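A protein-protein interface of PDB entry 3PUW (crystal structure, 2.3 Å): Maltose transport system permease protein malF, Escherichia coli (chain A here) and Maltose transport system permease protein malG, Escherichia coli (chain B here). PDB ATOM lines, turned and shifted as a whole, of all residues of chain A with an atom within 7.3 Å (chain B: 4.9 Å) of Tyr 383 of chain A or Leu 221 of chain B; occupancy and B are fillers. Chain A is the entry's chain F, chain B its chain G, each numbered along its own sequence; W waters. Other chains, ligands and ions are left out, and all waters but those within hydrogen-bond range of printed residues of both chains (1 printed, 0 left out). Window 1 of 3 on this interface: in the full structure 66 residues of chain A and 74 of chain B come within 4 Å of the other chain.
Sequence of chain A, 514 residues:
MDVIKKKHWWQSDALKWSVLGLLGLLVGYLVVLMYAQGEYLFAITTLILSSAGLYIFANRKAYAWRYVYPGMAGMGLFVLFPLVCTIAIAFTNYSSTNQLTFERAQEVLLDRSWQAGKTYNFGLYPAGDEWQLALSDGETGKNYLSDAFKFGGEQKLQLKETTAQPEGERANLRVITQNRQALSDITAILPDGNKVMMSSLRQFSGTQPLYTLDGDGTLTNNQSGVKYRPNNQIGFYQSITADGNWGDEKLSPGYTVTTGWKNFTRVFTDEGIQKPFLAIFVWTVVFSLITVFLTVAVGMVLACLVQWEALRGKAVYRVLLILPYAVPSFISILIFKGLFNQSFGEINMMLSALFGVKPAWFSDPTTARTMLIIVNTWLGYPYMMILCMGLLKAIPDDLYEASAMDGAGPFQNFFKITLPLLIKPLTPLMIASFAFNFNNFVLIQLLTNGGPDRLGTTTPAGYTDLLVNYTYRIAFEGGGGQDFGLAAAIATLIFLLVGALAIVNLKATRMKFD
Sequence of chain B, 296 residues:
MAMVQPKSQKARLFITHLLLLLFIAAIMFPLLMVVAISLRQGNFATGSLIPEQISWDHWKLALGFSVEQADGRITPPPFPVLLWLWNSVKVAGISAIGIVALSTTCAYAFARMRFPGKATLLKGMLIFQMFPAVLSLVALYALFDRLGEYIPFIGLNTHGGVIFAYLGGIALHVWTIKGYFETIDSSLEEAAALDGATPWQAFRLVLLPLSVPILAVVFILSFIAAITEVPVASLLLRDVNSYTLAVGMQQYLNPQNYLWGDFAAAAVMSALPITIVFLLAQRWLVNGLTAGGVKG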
ATOM      1  N   THR A 295      29.034  15.013  -3.989  1.00  0.00           N
ATOM      2  CA  THR A 295      28.488  13.773  -3.420  1.00  0.00           C
ATOM      3  C   THR A 295      27.350  14.042  -2.431  1.00  0.00           C
ATOM      4  O   THR A 295      26.330  13.353  -2.459  1.00  0.00           O
ATOM      5  CB  THR A 295      29.573  12.873  -2.768  1.00  0.00           C
ATOM      6  OG1 THR A 295      30.358  13.642  -1.848  1.00  0.00           O
ATOM      7  CG2 THR A 295      30.487  12.270  -3.832  1.00  0.00           C
ATOM      8  N   GLY A 299      23.690  12.928  -3.523  1.00  0.00           N
ATOM      9  CA  GLY A 299      23.165  11.955  -2.573  1.00  0.00           C
ATOM     10  C   GLY A 299      21.939  12.435  -1.818  1.00  0.00           C
ATOM     11  O   GLY A 299      20.982  11.672  -1.636  1.00  0.00           O
ATOM     12  N   ILE A 322      22.412   2.614  -5.449  1.00  0.00           N
ATOM     13  CA  ILE A 322      23.521   2.301  -4.543  1.00  0.00           C
ATOM     14  C   ILE A 322      24.478   1.224  -5.078  1.00  0.00           C
ATOM     15  O   ILE A 322      25.482   0.901  -4.435  1.00  0.00           O
ATOM     16  CB  ILE A 322      23.022   1.920  -3.113  1.00  0.00           C
ATOM     17  CG1 ILE A 322      22.048   0.733  -3.143  1.00  0.00           C
ATOM     18  CG2 ILE A 322      22.359   3.121  -2.426  1.00  0.00           C
ATOM     19  CD1 ILE A 322      22.708  -0.628  -3.050  1.00  0.00           C
ATOM     20  N   TYR A 325      28.234   1.345  -5.276  1.00  0.00           N
ATOM     21  CA  TYR A 325      28.869   1.166  -3.981  1.00  0.00           C
ATOM     22  C   TYR A 325      28.843  -0.304  -3.552  1.00  0.00           C
ATOM     23  O   TYR A 325      29.559  -0.695  -2.638  1.00  0.00           O
ATOM     24  CB  TYR A 325      28.144   2.045  -2.964  1.00  0.00           C
ATOM     25  CG  TYR A 325      28.865   2.315  -1.658  1.00  0.00           C
ATOM     26  CD1 TYR A 325      30.268   2.360  -1.582  1.00  0.00           C
ATOM     27  CD2 TYR A 325      28.131   2.571  -0.496  1.00  0.00           C
ATOM     28  CE1 TYR A 325      30.904   2.625  -0.371  1.00  0.00           C
ATOM     29  CE2 TYR A 325      28.754   2.837   0.703  1.00  0.00           C
ATOM     30  CZ  TYR A 325      30.135   2.865   0.765  1.00  0.00           C
ATOM     31  OH  TYR A 325      30.721   3.136   1.979  1.00  0.00           O
ATOM     32  N   TRP A 378      30.723   9.486  -8.767  1.00  0.00           N
ATOM     33  CA  TRP A 378      30.065   8.213  -9.062  1.00  0.00           C
ATOM     34  C   TRP A 378      30.365   7.217  -7.944  1.00  0.00           C
ATOM     35  O   TRP A 378      29.479   6.488  -7.496  1.00  0.00           O
ATOM     36  CB  TRP A 378      30.552   7.674 -10.410  1.00  0.00           C
ATOM     37  CG  TRP A 378      29.878   6.413 -10.877  1.00  0.00           C
ATOM     38  CD1 TRP A 378      28.779   6.323 -11.686  1.00  0.00           C
ATOM     39  CD2 TRP A 378      30.269   5.064 -10.582  1.00  0.00           C
ATOM     40  NE1 TRP A 378      28.463   5.004 -11.912  1.00  0.00           N
ATOM     41  CE2 TRP A 378      29.356   4.209 -11.243  1.00  0.00           C
ATOM     42  CE3 TRP A 378      31.309   4.491  -9.827  1.00  0.00           C
ATOM     43  CZ2 TRP A 378      29.447   2.814 -11.170  1.00  0.00           C
ATOM     44  CZ3 TRP A 378      31.399   3.107  -9.756  1.00  0.00           C
ATOM     45  CH2 TRP A 378      30.472   2.284 -10.427  1.00  0.00           C
ATOM     46  N   LEU A 379      31.620   7.199  -7.500  1.00  0.00           N
ATOM     47  CA  LEU A 379      32.052   6.334  -6.409  1.00  0.00           C
ATOM     48  C   LEU A 379      31.398   6.699  -5.073  1.00  0.00           C
ATOM     49  O   LEU A 379      30.983   5.812  -4.320  1.00  0.00           O
ATOM     50  CB  LEU A 379      33.579   6.382  -6.258  1.00  0.00           C
ATOM     51  CG  LEU A 379      34.462   5.698  -7.309  1.00  0.00           C
ATOM     52  CD1 LEU A 379      35.920   6.065  -7.099  1.00  0.00           C
ATOM     53  CD2 LEU A 379      34.280   4.191  -7.283  1.00  0.00           C
ATOM     54  N   GLY A 380      31.291   7.999  -4.795  1.00  0.00           N
ATOM     55  CA  GLY A 380      30.971   8.472  -3.452  1.00  0.00           C
ATOM     56  C   GLY A 380      29.563   8.937  -3.121  1.00  0.00           C
ATOM     57  O   GLY A 380      29.250   9.148  -1.940  1.00  0.00           O
ATOM     58  N   TYR A 381      28.712   9.106  -4.133  1.00  0.00           N
ATOM     59  CA  TYR A 381      27.348   9.590  -3.883  1.00  0.00           C
ATOM     60  C   TYR A 381      26.470   8.625  -3.057  1.00  0.00           C
ATOM     61  O   TYR A 381      25.654   9.091  -2.263  1.00  0.00           O
ATOM     62  CB  TYR A 381      26.632  10.060  -5.169  1.00  0.00           C
ATOM     63  CG  TYR A 381      25.981   8.968  -5.993  1.00  0.00           C
ATOM     64  CD1 TYR A 381      24.775   8.379  -5.591  1.00  0.00           C
ATOM     65  CD2 TYR A 381      26.562   8.533  -7.184  1.00  0.00           C
ATOM     66  CE1 TYR A 381      24.178   7.375  -6.344  1.00  0.00           C
ATOM     67  CE2 TYR A 381      25.976   7.530  -7.946  1.00  0.00           C
ATOM     68  CZ  TYR A 381      24.786   6.956  -7.524  1.00  0.00           C
ATOM     69  OH  TYR A 381      24.211   5.962  -8.280  1.00  0.00           O
ATOM     70  N   PRO A 382      26.629   7.289  -3.241  1.00  0.00           N
ATOM     71  CA  PRO A 382      25.795   6.375  -2.460  1.00  0.00           C
ATOM     72  C   PRO A 382      26.060   6.443  -0.954  1.00  0.00           C
ATOM     73  O   PRO A 382      25.132   6.269  -0.158  1.00  0.00           O
ATOM     74  CB  PRO A 382      26.174   4.997  -3.019  1.00  0.00           C
ATOM     75  CG  PRO A 382      26.632   5.279  -4.412  1.00  0.00           C
ATOM     76  CD  PRO A 382      27.409   6.550  -4.257  1.00  0.00           C
ATOM     77  N   TYR A 383      27.313   6.699  -0.576  1.00  0.00           N
ATOM     78  CA  TYR A 383      27.669   6.914   0.822  1.00  0.00           C
ATOM     79  C   TYR A 383      26.790   8.002   1.440  1.00  0.00           C
ATOM     80  O   TYR A 383      26.141   7.780   2.471  1.00  0.00           O
ATOM     81  CB  TYR A 383      29.144   7.293   0.953  1.00  0.00           C
ATOM     82  CG  TYR A 383      29.571   7.569   2.376  1.00  0.00           C
ATOM     83  CD1 TYR A 383      29.638   6.539   3.317  1.00  0.00           C
ATOM     84  CD2 TYR A 383      29.904   8.859   2.789  1.00  0.00           C
ATOM     85  CE1 TYR A 383      30.023   6.787   4.633  1.00  0.00           C
ATOM     86  CE2 TYR A 383      30.299   9.113   4.105  1.00  0.00           C
ATOM     87  CZ  TYR A 383      30.357   8.073   5.018  1.00  0.00           C
ATOM     88  OH  TYR A 383      30.736   8.319   6.320  1.00  0.00           O
ATOM     89  N   MET A 384      26.764   9.164   0.789  1.00  0.00           N
ATOM     90  CA  MET A 384      25.971  10.300   1.242  1.00  0.00           C
ATOM     91  C   MET A 384      24.479  10.047   1.107  1.00  0.00           C
ATOM     92  O   MET A 384      23.706  10.464   1.967  1.00  0.00           O
ATOM     93  CB  MET A 384      26.361  11.566   0.484  1.00  0.00           C
ATOM     94  CG  MET A 384      27.763  12.049   0.786  1.00  0.00           C
ATOM     95  SD  MET A 384      27.988  12.454   2.530  1.00  0.00           S
ATOM     96  CE  MET A 384      29.775  12.591   2.563  1.00  0.00           C
ATOM     97  N   MET A 385      24.081   9.365   0.035  1.00  0.00           N
ATOM     98  CA  MET A 385      22.679   9.010  -0.185  1.00  0.00           C
ATOM     99  C   MET A 385      22.130   8.177   0.973  1.00  0.00           C
ATOM    100  O   MET A 385      21.069   8.484   1.519  1.00  0.00           O
ATOM    101  CB  MET A 385      22.492   8.261  -1.516  1.00  0.00           C
ATOM    102  CG  MET A 385      21.022   7.970  -1.847  1.00  0.00           C
ATOM    103  SD  MET A 385      20.768   6.813  -3.207  1.00  0.00           S
ATOM    104  CE  MET A 385      18.980   6.730  -3.246  1.00  0.00           C
ATOM    105  N   ILE A 386      22.870   7.136   1.345  1.00  0.00           N
ATOM    106  CA  ILE A 386      22.447   6.210   2.394  1.00  0.00           C
ATOM    107  C   ILE A 386      22.299   6.926   3.743  1.00  0.00           C
ATOM    108  O   ILE A 386      21.331   6.698   4.475  1.00  0.00           O
ATOM    109  CB  ILE A 386      23.413   4.988   2.481  1.00  0.00           C
ATOM    110  CG1 ILE A 386      23.251   4.096   1.237  1.00  0.00           C
ATOM    111  CG2 ILE A 386      23.163   4.176   3.752  1.00  0.00           C
ATOM    112  CD1 ILE A 386      24.409   3.134   0.982  1.00  0.00           C
ATOM    113  N   LEU A 387      23.257   7.798   4.051  1.00  0.00           N
ATOM    114  CA  LEU A 387      23.220   8.615   5.257  1.00  0.00           C
ATOM    115  C   LEU A 387      21.962   9.477   5.297  1.00  0.00           C
ATOM    116  O   LEU A 387      21.216   9.446   6.275  1.00  0.00           O
ATOM    117  CB  LEU A 387      24.465   9.496   5.345  1.00  0.00           C
ATOM    118  CG  LEU A 387      25.781   8.820   5.729  1.00  0.00           C
ATOM    119  CD1 LEU A 387      26.931   9.735   5.359  1.00  0.00           C
ATOM    120  CD2 LEU A 387      25.815   8.458   7.221  1.00  0.00           C
ATOM    121  N   CYS A 388      21.725  10.228   4.226  1.00  0.00           N
ATOM    122  CA  CYS A 388      20.559  11.095   4.136  1.00  0.00           C
ATOM    123  C   CYS A 388      19.253  10.303   4.211  1.00  0.00           C
ATOM    124  O   CYS A 388      18.288  10.756   4.826  1.00  0.00           O
ATOM    125  CB  CYS A 388      20.620  11.957   2.873  1.00  0.00           C
ATOM    126  SG  CYS A 388      21.966  13.173   2.892  1.00  0.00           S
ATOM    127  N   MET A 389      19.241   9.108   3.621  1.00  0.00           N
ATOM    128  CA  MET A 389      18.076   8.219   3.682  1.00  0.00           C
ATOM    129  C   MET A 389      17.613   7.987   5.117  1.00  0.00           C
ATOM    130  O   MET A 389      16.416   7.979   5.395  1.00  0.00           O
ATOM    131  CB  MET A 389      18.376   6.873   3.023  1.00  0.00           C
ATOM    132  CG  MET A 389      18.353   6.897   1.505  1.00  0.00           C
ATOM    133  SD  MET A 389      18.752   5.296   0.773  1.00  0.00           S
ATOM    134  CE  MET A 389      17.363   4.308   1.350  1.00  0.00           C
ATOM    135  N   LEU A 429      30.385  14.420   9.185  1.00  0.00           N
ATOM    136  CA  LEU A 429      30.552  13.460   8.098  1.00  0.00           C
ATOM    137  C   LEU A 429      31.204  14.085   6.875  1.00  0.00           C
ATOM    138  O   LEU A 429      31.968  13.422   6.176  1.00  0.00           O
ATOM    139  CB  LEU A 429      29.215  12.826   7.722  1.00  0.00           C
ATOM    140  CG  LEU A 429      28.630  11.895   8.787  1.00  0.00           C
ATOM    141  CD1 LEU A 429      27.146  11.663   8.549  1.00  0.00           C
ATOM    142  CD2 LEU A 429      29.392  10.572   8.866  1.00  0.00           C
ATOM    143  N   MET A 430      30.910  15.360   6.636  1.00  0.00           N
ATOM    144  CA  MET A 430      31.500  16.107   5.525  1.00  0.00           C
ATOM    145  C   MET A 430      32.957  16.471   5.790  1.00  0.00           C
ATOM    146  O   MET A 430      33.779  16.446   4.874  1.00  0.00           O
ATOM    147  CB  MET A 430      30.684  17.366   5.220  1.00  0.00           C
ATOM    148  CG  MET A 430      29.341  17.077   4.561  1.00  0.00           C
ATOM    149  SD  MET A 430      28.270  18.523   4.439  1.00  0.00           S
ATOM    150  CE  MET A 430      29.118  19.457   3.163  1.00  0.00           C
ATOM    151  N   ALA A 432      34.905  14.701   7.679  1.00  0.00           N
ATOM    152  CA  ALA A 432      35.565  13.403   7.546  1.00  0.00           C
ATOM    153  C   ALA A 432      35.775  13.041   6.079  1.00  0.00           C
ATOM    154  O   ALA A 432      36.862  12.612   5.688  1.00  0.00           O
ATOM    155  CB  ALA A 432      34.763  12.333   8.244  1.00  0.00           C
ATOM    156  N   SER A 433      34.729  13.223   5.274  1.00  0.00           N
ATOM    157  CA  SER A 433      34.801  12.963   3.836  1.00  0.00           C
ATOM    158  C   SER A 433      35.850  13.835   3.146  1.00  0.00           C
ATOM    159  O   SER A 433      36.440  13.418   2.155  1.00  0.00           O
ATOM    160  CB  SER A 433      33.433  13.153   3.177  1.00  0.00           C
ATOM    161  OG  SER A 433      33.453  12.738   1.821  1.00  0.00           O
ATOM    162  N   LEU B 172      33.137   7.596  13.390  1.00  0.00           N
ATOM    163  CA  LEU B 172      32.158   8.277  12.547  1.00  0.00           C
ATOM    164  C   LEU B 172      30.738   7.816  12.847  1.00  0.00           C
ATOM    165  O   LEU B 172      29.822   8.639  12.963  1.00  0.00           O
ATOM    166  CB  LEU B 172      32.494   8.087  11.065  1.00  0.00           C
ATOM    167  CG  LEU B 172      33.486   9.095  10.478  1.00  0.00           C
ATOM    168  CD1 LEU B 172      33.926   8.676   9.096  1.00  0.00           C
ATOM    169  CD2 LEU B 172      32.850  10.479  10.441  1.00  0.00           C
ATOM    170  N   HIS B 173      30.568   6.504  12.992  1.00  0.00           N
ATOM    171  CA  HIS B 173      29.276   5.920  13.334  1.00  0.00           C
ATOM    172  C   HIS B 173      28.763   6.444  14.673  1.00  0.00           C
ATOM    173  O   HIS B 173      27.563   6.682  14.828  1.00  0.00           O
ATOM    174  CB  HIS B 173      29.351   4.391  13.341  1.00  0.00           C
ATOM    175  CG  HIS B 173      29.725   3.800  12.017  1.00  0.00           C
ATOM    176  ND1 HIS B 173      29.050   4.098  10.852  1.00  0.00           N
ATOM    177  CD2 HIS B 173      30.697   2.921  11.674  1.00  0.00           C
ATOM    178  CE1 HIS B 173      29.595   3.434   9.848  1.00  0.00           C
ATOM    179  NE2 HIS B 173      30.594   2.710  10.320  1.00  0.00           N
ATOM    180  N   VAL B 217      21.136   2.430   8.805  1.00  0.00           N
ATOM    181  CA  VAL B 217      22.200   3.117   8.069  1.00  0.00           C
ATOM    182  C   VAL B 217      23.576   2.586   8.478  1.00  0.00           C
ATOM    183  O   VAL B 217      24.364   2.155   7.627  1.00  0.00           O
ATOM    184  CB  VAL B 217      22.143   4.657   8.279  1.00  0.00           C
ATOM    185  CG1 VAL B 217      23.483   5.337   7.926  1.00  0.00           C
ATOM    186  CG2 VAL B 217      20.997   5.261   7.488  1.00  0.00           C
ATOM    187  N   VAL B 218      23.854   2.604   9.778  1.00  0.00           N
ATOM    188  CA  VAL B 218      25.161   2.188  10.284  1.00  0.00           C
ATOM    189  C   VAL B 218      25.431   0.708   9.995  1.00  0.00           C
ATOM    190  O   VAL B 218      26.570   0.334   9.700  1.00  0.00           O
ATOM    191  CB  VAL B 218      25.334   2.521  11.790  1.00  0.00           C
ATOM    192  CG1 VAL B 218      26.629   1.933  12.337  1.00  0.00           C
ATOM    193  CG2 VAL B 218      25.312   4.029  12.005  1.00  0.00           C
ATOM    194  N   PHE B 219      24.384  -0.120  10.047  1.00  0.00           N
ATOM    195  CA  PHE B 219      24.515  -1.528   9.673  1.00  0.00           C
ATOM    196  C   PHE B 219      24.871  -1.671   8.194  1.00  0.00           C
ATOM    197  O   PHE B 219      25.801  -2.394   7.843  1.00  0.00           O
ATOM    198  CB  PHE B 219      23.247  -2.332   9.991  1.00  0.00           C
ATOM    199  CG  PHE B 219      23.420  -3.822   9.824  1.00  0.00           C
ATOM    200  CD1 PHE B 219      23.862  -4.608  10.885  1.00  0.00           C
ATOM    201  CD2 PHE B 219      23.157  -4.439   8.608  1.00  0.00           C
ATOM    202  CE1 PHE B 219      24.036  -5.986  10.737  1.00  0.00           C
ATOM    203  CE2 PHE B 219      23.336  -5.817   8.449  1.00  0.00           C
ATOM    204  CZ  PHE B 219      23.775  -6.591   9.517  1.00  0.00           C
ATOM    205  N   ILE B 220      24.122  -0.984   7.335  1.00  0.00           N
ATOM    206  CA  ILE B 220      24.359  -1.027   5.891  1.00  0.00           C
ATOM    207  C   ILE B 220      25.787  -0.615   5.571  1.00  0.00           C
ATOM    208  O   ILE B 220      26.522  -1.373   4.928  1.00  0.00           O
ATOM    209  CB  ILE B 220      23.389  -0.108   5.127  1.00  0.00           C
ATOM    210  CG1 ILE B 220      21.972  -0.688   5.152  1.00  0.00           C
ATOM    211  CG2 ILE B 220      23.877   0.124   3.687  1.00  0.00           C
ATOM    212  CD1 ILE B 220      20.901   0.333   4.823  1.00  0.00           C
ATOM    213  N   LEU B 221      26.171   0.576   6.034  1.00  0.00           N
ATOM    214  CA  LEU B 221      27.487   1.138   5.755  1.00  0.00           C
ATOM    215  C   LEU B 221      28.623   0.236   6.220  1.00  0.00           C
ATOM    216  O   LEU B 221      29.628   0.108   5.529  1.00  0.00           O
ATOM    217  CB  LEU B 221      27.622   2.538   6.353  1.00  0.00           C
ATOM    218  CG  LEU B 221      26.882   3.683   5.642  1.00  0.00           C
ATOM    219  CD1 LEU B 221      27.003   4.968   6.430  1.00  0.00           C
ATOM    220  CD2 LEU B 221      27.384   3.904   4.215  1.00  0.00           C
ATOM    221  N   SER B 222      28.446  -0.400   7.376  1.00  0.00           N
ATOM    222  CA  SER B 222      29.442  -1.323   7.931  1.00  0.00           C
ATOM    223  C   SER B 222      29.522  -2.620   7.147  1.00  0.00           C
ATOM    224  O   SER B 222      30.616  -3.112   6.875  1.00  0.00           O
ATOM    225  CB  SER B 222      29.130  -1.639   9.386  1.00  0.00           C
ATOM    226  OG  SER B 222      29.020  -0.442  10.114  1.00  0.00           O
ATOM    227  N   PHE B 223      28.361  -3.169   6.794  1.00  0.00           N
ATOM    228  CA  PHE B 223      28.299  -4.366   5.970  1.00  0.00           C
ATOM    229  C   PHE B 223      29.052  -4.163   4.644  1.00  0.00           C
ATOM    230  O   PHE B 223      29.889  -4.980   4.279  1.00  0.00           O
ATOM    231  CB  PHE B 223      26.850  -4.777   5.726  1.00  0.00           C
ATOM    232  CG  PHE B 223      26.697  -6.186   5.241  1.00  0.00           C
ATOM    233  CD1 PHE B 223      26.562  -7.233   6.145  1.00  0.00           C
ATOM    234  CD2 PHE B 223      26.685  -6.470   3.879  1.00  0.00           C
ATOM    235  CE1 PHE B 223      26.414  -8.546   5.703  1.00  0.00           C
ATOM    236  CE2 PHE B 223      26.537  -7.775   3.427  1.00  0.00           C
ATOM    237  CZ  PHE B 223      26.407  -8.819   4.342  1.00  0.00           C
ATOM    238  N   ILE B 224      28.767  -3.060   3.951  1.00  0.00           N
ATOM    239  CA  ILE B 224      29.450  -2.706   2.698  1.00  0.00           C
ATOM    240  C   ILE B 224      30.963  -2.607   2.892  1.00  0.00           C
ATOM    241  O   ILE B 224      31.732  -3.183   2.119  1.00  0.00           O
ATOM    242  CB  ILE B 224      28.908  -1.382   2.101  1.00  0.00           C
ATOM    243  CG1 ILE B 224      27.444  -1.543   1.699  1.00  0.00           C
ATOM    244  CG2 ILE B 224      29.726  -0.943   0.896  1.00  0.00           C
ATOM    245  CD1 ILE B 224      26.752  -0.244   1.376  1.00  0.00           C
ATOM    246  N   ALA B 225      31.377  -1.886   3.933  1.00  0.00           N
ATOM    247  CA  ALA B 225      32.792  -1.733   4.273  1.00  0.00           C
ATOM    248  C   ALA B 225      33.477  -3.090   4.419  1.00  0.00           C
ATOM    249  O   ALA B 225      34.531  -3.327   3.824  1.00  0.00           O
ATOM    250  CB  ALA B 225      32.949  -0.919   5.539  1.00  0.00           C
HETATM  251  O   HOH W   1      30.923   2.035   4.270  1.00  0.00           O
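Of chain B, only Leu 221 (3.6 Å) comes within 4 Å of Tyr 383 of chain A. Of chain A, only Tyr 325, Tyr 383 and Leu 387 come within 4 Å of Leu 221 of chain B. Printed residues of chain A within 4 Å of Val 217 of chain B: Ile 386 and Leu 387. Printed residues of chain B within 4 Å of Ala 432 of chain A: Leu 172 (3.5 Å). Of the printed residues of chain B, Leu 387 of chain A touches Val 217 and Leu 221. Printed residues of chain B within 4 Å of Ile 386 of chain A: Val 217. Printed residues of chain B within 4 Å of Leu 429 of chain A: Leu 172. Phe 219 of chain B touches none of the printed residues of chain A.
Tyr 325 of chain A touches Leu 221 of chain B (CE2 to CD2, 3.9 Å). Tyr 325 of chain A touches Ile 224 of chain B (O to CG2, 3.5 Å). Tyr 383 of chain A touches Leu 221 of chain B. Ile 386 of chain A touches Val 217 of chain B (O to CG2, 3.4 Å). CD2 of Leu 387 of chain A touches CG1 of Val 217 of chain B, 3.96 Å away. Leu 387 of chain A touches Leu 221 of chain B. Leu 429 of chain A touches Leu 172 of chain B. Ala 432 of chain A touches Leu 172 of chain B.
Water W1 lies within hydrogen-bond range of OH of Tyr 325 of chain A (2.5 Å) and O of Leu 221 of chain B (2.6 Å).
Hydrophobic or aromatic side chains of chain A that line the printed part of chain B: Tyr 325, Tyr 383, Leu 387, Leu 429 and Ala 432. Of the 11 printed residues of chain B, 4 touch a printed residue of chain A. Hydrophobic or aromatic side chains of chain B that line the printed part of chain A: Leu 172, Val 217, Leu 221 and Ile 224. Along chain B the printed residues that touch a printed residue of chain A span positions 172 to 224. Among the printed residues, no Asp or Glu carboxylate lies within 4 Å of a Lys or Arg side-chain nitrogen of the other chain.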
